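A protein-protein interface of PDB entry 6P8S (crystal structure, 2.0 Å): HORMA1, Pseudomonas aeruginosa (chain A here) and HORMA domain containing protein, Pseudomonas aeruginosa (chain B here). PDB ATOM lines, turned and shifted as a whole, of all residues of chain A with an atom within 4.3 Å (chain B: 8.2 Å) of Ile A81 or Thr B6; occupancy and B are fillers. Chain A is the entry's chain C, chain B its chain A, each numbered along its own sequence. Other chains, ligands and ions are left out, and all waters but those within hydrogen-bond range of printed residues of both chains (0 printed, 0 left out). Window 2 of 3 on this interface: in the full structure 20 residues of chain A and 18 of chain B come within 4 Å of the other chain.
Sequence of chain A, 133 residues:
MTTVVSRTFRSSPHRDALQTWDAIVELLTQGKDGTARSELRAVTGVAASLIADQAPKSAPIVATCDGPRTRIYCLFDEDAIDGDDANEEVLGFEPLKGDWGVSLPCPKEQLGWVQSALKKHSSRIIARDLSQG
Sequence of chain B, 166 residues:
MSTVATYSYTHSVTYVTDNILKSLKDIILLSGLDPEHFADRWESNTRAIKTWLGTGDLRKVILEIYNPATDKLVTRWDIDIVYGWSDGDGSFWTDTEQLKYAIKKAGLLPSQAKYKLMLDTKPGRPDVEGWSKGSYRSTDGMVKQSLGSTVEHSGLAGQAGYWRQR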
ATOM      1  N   PRO A  13     -11.737  12.928  20.485  1.00  0.00           N
ATOM      2  CA  PRO A  13     -10.539  12.601  19.701  1.00  0.00           C
ATOM      3  C   PRO A  13     -10.490  11.206  19.078  1.00  0.00           C
ATOM      4  O   PRO A  13      -9.453  10.855  18.507  1.00  0.00           O
ATOM      5  CB  PRO A  13      -9.415  12.733  20.746  1.00  0.00           C
ATOM      6  CG  PRO A  13     -10.087  12.201  22.007  1.00  0.00           C
ATOM      7  CD  PRO A  13     -11.554  12.620  21.917  1.00  0.00           C
ATOM      8  N   ASP A  77     -14.295  13.465  23.646  1.00  0.00           N
ATOM      9  CA  ASP A  77     -13.379  13.349  24.794  1.00  0.00           C
ATOM     10  C   ASP A  77     -13.500  11.936  25.370  1.00  0.00           C
ATOM     11  O   ASP A  77     -13.505  10.966  24.598  1.00  0.00           O
ATOM     12  CB  ASP A  77     -13.682  14.473  25.760  1.00  0.00           C
ATOM     13  CG  ASP A  77     -13.597  15.836  25.104  1.00  0.00           C
ATOM     14  OD1 ASP A  77     -12.778  15.999  24.165  1.00  0.00           O
ATOM     15  OD2 ASP A  77     -14.350  16.742  25.524  1.00  0.00           O
ATOM     16  N   GLU A  78     -13.564  11.788  26.697  1.00  0.00           N
ATOM     17  CA  GLU A  78     -13.532  10.453  27.285  1.00  0.00           C
ATOM     18  C   GLU A  78     -14.650   9.578  26.730  1.00  0.00           C
ATOM     19  O   GLU A  78     -14.467   8.369  26.540  1.00  0.00           O
ATOM     20  CB  GLU A  78     -13.636  10.539  28.810  1.00  0.00           C
ATOM     21  CG  GLU A  78     -12.511  11.291  29.494  1.00  0.00           C
ATOM     22  CD  GLU A  78     -12.866  12.747  29.766  1.00  0.00           C
ATOM     23  OE1 GLU A  78     -13.703  13.308  29.014  1.00  0.00           O
ATOM     24  OE2 GLU A  78     -12.312  13.325  30.732  1.00  0.00           O
ATOM     25  N   ASP A  79     -15.818  10.170  26.471  1.00  0.00           N
ATOM     26  CA  ASP A  79     -16.940   9.394  25.960  1.00  0.00           C
ATOM     27  C   ASP A  79     -16.647   8.840  24.569  1.00  0.00           C
ATOM     28  O   ASP A  79     -17.078   7.726  24.239  1.00  0.00           O
ATOM     29  CB  ASP A  79     -18.203  10.254  25.935  1.00  0.00           C
ATOM     30  CG  ASP A  79     -18.603  10.749  27.316  1.00  0.00           C
ATOM     31  OD1 ASP A  79     -18.261  10.086  28.316  1.00  0.00           O
ATOM     32  OD2 ASP A  79     -19.261  11.805  27.396  1.00  0.00           O
ATOM     33  N   ALA A  80     -15.921   9.602  23.744  1.00  0.00           N
ATOM     34  CA  ALA A  80     -15.617   9.143  22.394  1.00  0.00           C
ATOM     35  C   ALA A  80     -14.616   7.995  22.412  1.00  0.00           C
ATOM     36  O   ALA A  80     -14.761   7.027  21.659  1.00  0.00           O
ATOM     37  CB  ALA A  80     -15.098  10.310  21.551  1.00  0.00           C
ATOM     38  N   ILE A  81     -13.594   8.086  23.262  1.00  0.00           N
ATOM     39  CA  ILE A  81     -12.639   6.994  23.393  1.00  0.00           C
ATOM     40  C   ILE A  81     -13.315   5.774  23.999  1.00  0.00           C
ATOM     41  O   ILE A  81     -13.108   4.646  23.541  1.00  0.00           O
ATOM     42  CB  ILE A  81     -11.432   7.453  24.229  1.00  0.00           C
ATOM     43  CG1 ILE A  81     -10.730   8.632  23.544  1.00  0.00           C
ATOM     44  CG2 ILE A  81     -10.465   6.301  24.449  1.00  0.00           C
ATOM     45  CD1 ILE A  81      -9.725   9.346  24.423  1.00  0.00           C
ATOM     46  N   ASP A  82     -14.127   5.979  25.041  1.00  0.00           N
ATOM     47  CA  ASP A  82     -14.881   4.882  25.641  1.00  0.00           C
ATOM     48  C   ASP A  82     -15.747   4.183  24.602  1.00  0.00           C
ATOM     49  O   ASP A  82     -15.603   2.979  24.362  1.00  0.00           O
ATOM     50  CB  ASP A  82     -15.758   5.408  26.781  1.00  0.00           C
ATOM     51  CG  ASP A  82     -14.968   5.738  28.025  1.00  0.00           C
ATOM     52  OD1 ASP A  82     -13.926   5.082  28.257  1.00  0.00           O
ATOM     53  OD2 ASP A  82     -15.397   6.637  28.785  1.00  0.00           O
ATOM     54  N   GLY A  83     -16.668   4.924  23.990  1.00  0.00           N
ATOM     55  CA  GLY A  83     -17.652   4.360  23.098  1.00  0.00           C
ATOM     56  C   GLY A  83     -18.871   3.789  23.783  1.00  0.00           C
ATOM     57  O   GLY A  83     -19.751   3.256  23.096  1.00  0.00           O
ATOM     58  N   ALA B   5      -8.221   7.742  31.979  1.00  0.00           N
ATOM     59  CA  ALA B   5      -8.190   6.404  31.392  1.00  0.00           C
ATOM     60  C   ALA B   5      -7.111   6.320  30.312  1.00  0.00           C
ATOM     61  O   ALA B   5      -6.235   7.185  30.225  1.00  0.00           O
ATOM     62  CB  ALA B   5      -9.554   6.038  30.816  1.00  0.00           C
ATOM     63  N   THR B   6      -7.179   5.281  29.484  1.00  0.00           N
ATOM     64  CA  THR B   6      -6.154   5.060  28.478  1.00  0.00           C
ATOM     65  C   THR B   6      -6.422   5.902  27.237  1.00  0.00           C
ATOM     66  O   THR B   6      -7.568   6.069  26.812  1.00  0.00           O
ATOM     67  CB  THR B   6      -6.079   3.583  28.093  1.00  0.00           C
ATOM     68  OG1 THR B   6      -5.886   2.791  29.271  1.00  0.00           O
ATOM     69  CG2 THR B   6      -4.925   3.340  27.133  1.00  0.00           C
ATOM     70  N   TYR B   7      -5.345   6.427  26.662  1.00  0.00           N
ATOM     71  CA  TYR B   7      -5.392   7.207  25.441  1.00  0.00           C
ATOM     72  C   TYR B   7      -4.139   6.886  24.641  1.00  0.00           C
ATOM     73  O   TYR B   7      -3.191   6.277  25.146  1.00  0.00           O
ATOM     74  CB  TYR B   7      -5.465   8.701  25.732  1.00  0.00           C
ATOM     75  CG  TYR B   7      -4.265   9.175  26.502  1.00  0.00           C
ATOM     76  CD1 TYR B   7      -4.217   9.057  27.889  1.00  0.00           C
ATOM     77  CD2 TYR B   7      -3.167   9.717  25.851  1.00  0.00           C
ATOM     78  CE1 TYR B   7      -3.115   9.481  28.603  1.00  0.00           C
ATOM     79  CE2 TYR B   7      -2.061  10.145  26.555  1.00  0.00           C
ATOM     80  CZ  TYR B   7      -2.038  10.019  27.931  1.00  0.00           C
ATOM     81  OH  TYR B   7      -0.941  10.449  28.645  1.00  0.00           O
ATOM     82  N   SER B   8      -4.142   7.298  23.381  1.00  0.00           N
ATOM     83  CA  SER B   8      -3.022   7.055  22.485  1.00  0.00           C
ATOM     84  C   SER B   8      -2.507   8.379  21.945  1.00  0.00           C
ATOM     85  O   SER B   8      -3.197   9.402  21.993  1.00  0.00           O
ATOM     86  CB  SER B   8      -3.428   6.138  21.322  1.00  0.00           C
ATOM     87  OG  SER B   8      -4.210   6.835  20.363  1.00  0.00           O
ATOM     88  N   TYR B   9      -1.277   8.348  21.422  1.00  0.00           N
ATOM     89  CA  TYR B   9      -0.728   9.539  20.785  1.00  0.00           C
ATOM     90  C   TYR B   9      -1.663  10.041  19.695  1.00  0.00           C
ATOM     91  O   TYR B   9      -1.826  11.250  19.517  1.00  0.00           O
ATOM     92  CB  TYR B   9       0.660   9.239  20.219  1.00  0.00           C
ATOM     93  CG  TYR B   9       1.327  10.449  19.616  1.00  0.00           C
ATOM     94  CD1 TYR B   9       1.702  11.525  20.415  1.00  0.00           C
ATOM     95  CD2 TYR B   9       1.582  10.523  18.253  1.00  0.00           C
ATOM     96  CE1 TYR B   9       2.307  12.645  19.870  1.00  0.00           C
ATOM     97  CE2 TYR B   9       2.190  11.637  17.701  1.00  0.00           C
ATOM     98  CZ  TYR B   9       2.549  12.695  18.519  1.00  0.00           C
ATOM     99  OH  TYR B   9       3.153  13.813  17.984  1.00  0.00           O
ATOM    100  N   THR B  10      -2.296   9.125  18.958  1.00  0.00           N
ATOM    101  CA  THR B  10      -3.211   9.548  17.900  1.00  0.00           C
ATOM    102  C   THR B  10      -4.413  10.288  18.470  1.00  0.00           C
ATOM    103  O   THR B  10      -4.955  11.186  17.815  1.00  0.00           O
ATOM    104  CB  THR B  10      -3.671   8.340  17.079  1.00  0.00           C
ATOM    105  OG1 THR B  10      -2.521   7.688  16.517  1.00  0.00           O
ATOM    106  CG2 THR B  10      -4.610   8.783  15.958  1.00  0.00           C
ATOM    107  N   HIS B  11      -4.858   9.917  19.674  1.00  0.00           N
ATOM    108  CA  HIS B  11      -5.900  10.689  20.345  1.00  0.00           C
ATOM    109  C   HIS B  11      -5.427  12.113  20.606  1.00  0.00           C
ATOM    110  O   HIS B  11      -6.131  13.080  20.292  1.00  0.00           O
ATOM    111  CB  HIS B  11      -6.304  10.010  21.650  1.00  0.00           C
ATOM    112  CG  HIS B  11      -7.029   8.714  21.459  1.00  0.00           C
ATOM    113  ND1 HIS B  11      -6.787   7.604  22.241  1.00  0.00           N
ATOM    114  CD2 HIS B  11      -7.995   8.349  20.583  1.00  0.00           C
ATOM    115  CE1 HIS B  11      -7.563   6.610  21.847  1.00  0.00           C
ATOM    116  NE2 HIS B  11      -8.309   7.037  20.845  1.00  0.00           N
ATOM    117  N   SER B  12      -4.226  12.263  21.178  1.00  0.00           N
ATOM    118  CA  SER B  12      -3.678  13.597  21.414  1.00  0.00           C
ATOM    119  C   SER B  12      -3.539  14.372  20.112  1.00  0.00           C
ATOM    120  O   SER B  12      -3.858  15.570  20.055  1.00  0.00           O
ATOM    121  CB  SER B  12      -2.327  13.492  22.114  1.00  0.00           C
ATOM    122  OG  SER B  12      -2.457  12.945  23.418  1.00  0.00           O
ATOM    123  N   TYR B  15      -7.023  15.536  18.967  1.00  0.00           N
ATOM    124  CA  TYR B  15      -7.517  16.643  19.780  1.00  0.00           C
ATOM    125  C   TYR B  15      -6.859  17.959  19.374  1.00  0.00           C
ATOM    126  O   TYR B  15      -7.534  18.980  19.188  1.00  0.00           O
ATOM    127  CB  TYR B  15      -7.276  16.340  21.263  1.00  0.00           C
ATOM    128  CG  TYR B  15      -7.823  17.417  22.173  1.00  0.00           C
ATOM    129  CD1 TYR B  15      -7.085  18.565  22.442  1.00  0.00           C
ATOM    130  CD2 TYR B  15      -9.074  17.293  22.743  1.00  0.00           C
ATOM    131  CE1 TYR B  15      -7.587  19.567  23.250  1.00  0.00           C
ATOM    132  CE2 TYR B  15      -9.589  18.283  23.565  1.00  0.00           C
ATOM    133  CZ  TYR B  15      -8.840  19.413  23.818  1.00  0.00           C
ATOM    134  OH  TYR B  15      -9.338  20.406  24.628  1.00  0.00           O
ATOM    135  N   ASP B  87       2.653   9.408  27.838  1.00  0.00           N
ATOM    136  CA  ASP B  87       1.603   8.394  27.807  1.00  0.00           C
ATOM    137  C   ASP B  87       0.844   8.279  29.125  1.00  0.00           C
ATOM    138  O   ASP B  87      -0.229   7.657  29.150  1.00  0.00           O
ATOM    139  CB  ASP B  87       2.189   7.020  27.444  1.00  0.00           C
ATOM    140  CG  ASP B  87       3.066   6.441  28.549  1.00  0.00           C
ATOM    141  OD1 ASP B  87       3.374   7.170  29.516  1.00  0.00           O
ATOM    142  OD2 ASP B  87       3.435   5.255  28.448  1.00  0.00           O
ATOM    143  N   GLY B  90      -2.896  12.332  30.166  1.00  0.00           N
ATOM    144  CA  GLY B  90      -4.306  12.212  29.884  1.00  0.00           C
ATOM    145  C   GLY B  90      -5.101  13.502  29.931  1.00  0.00           C
ATOM    146  O   GLY B  90      -6.250  13.521  29.460  1.00  0.00           O
ATOM    147  N   PHE B  92      -6.334  17.345  29.081  1.00  0.00           N
ATOM    148  CA  PHE B  92      -6.503  18.081  27.837  1.00  0.00           C
ATOM    149  C   PHE B  92      -7.353  19.319  28.097  1.00  0.00           C
ATOM    150  O   PHE B  92      -8.194  19.335  28.997  1.00  0.00           O
ATOM    151  CB  PHE B  92      -7.167  17.205  26.759  1.00  0.00           C
ATOM    152  CG  PHE B  92      -8.487  16.631  27.192  1.00  0.00           C
ATOM    153  CD1 PHE B  92      -9.658  17.356  27.035  1.00  0.00           C
ATOM    154  CD2 PHE B  92      -8.556  15.370  27.770  1.00  0.00           C
ATOM    155  CE1 PHE B  92     -10.877  16.830  27.445  1.00  0.00           C
ATOM    156  CE2 PHE B  92      -9.776  14.849  28.194  1.00  0.00           C
ATOM    157  CZ  PHE B  92     -10.932  15.583  28.024  1.00  0.00           C
ATOM    158  N   HIS B 153      -3.158  18.350  24.645  1.00  0.00           N
ATOM    159  CA  HIS B 153      -3.652  17.032  25.033  1.00  0.00           C
ATOM    160  C   HIS B 153      -2.427  16.226  25.457  1.00  0.00           C
ATOM    161  O   HIS B 153      -1.631  15.798  24.614  1.00  0.00           O
ATOM    162  CB  HIS B 153      -4.413  16.341  23.913  1.00  0.00           C
ATOM    163  CG  HIS B 153      -5.160  15.123  24.365  1.00  0.00           C
ATOM    164  ND1 HIS B 153      -4.526  13.997  24.842  1.00  0.00           N
ATOM    165  CD2 HIS B 153      -6.486  14.857  24.413  1.00  0.00           C
ATOM    166  CE1 HIS B 153      -5.429  13.086  25.160  1.00  0.00           C
ATOM    167  NE2 HIS B 153      -6.627  13.583  24.911  1.00  0.00           N
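Of the 8 printed residues of chain A, 4 touch a printed residue of chain B.
Printed residues of chain B that touch a printed residue of chain A: Thr B6, His B11, Tyr B15 and Phe B92.
Hydrophobic or aromatic side chains of chain B within 4 Å of the printed part of chain A: His B11, Tyr B15 and Phe B92.
Among the printed residues, no Asp or Glu carboxylate lies within 4 Å of a Lys or Arg side-chain nitrogen of the other chain.
Among the printed residues, merely in contact across the chains: Pro A13 with His B11, Asp A77 with Tyr B15, Asp A77 with Phe B92, Glu A78 with Phe B92, Ile A81 with Thr B6 and Ile A81 with His B11.
The backbone NH of Ser B8 is in hydrogen-bond range of a ring nitrogen (ND1) of His B11, 2.9 Å away.
Printed residues of chain B within 4 Å of Ile A81: Thr B6 and His B11.
Thr B6 touches just one residue of chain A: Ile A81.
Of the printed residues of chain A, His B11 touches Pro A13 (3.3 Å) and Ile A81 (3.9 Å).
Of the printed residues of chain B, Asp A77 touches Tyr B15 and Phe B92.
Of the printed residues of chain B, Pro A13 touches His B11.
Printed residues of chain A within 4 Å of Phe B92: Asp A77 and Glu A78.
The nearest printed residue of chain A that does not touch Thr B6 is Asp A82 (6.6 Å).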
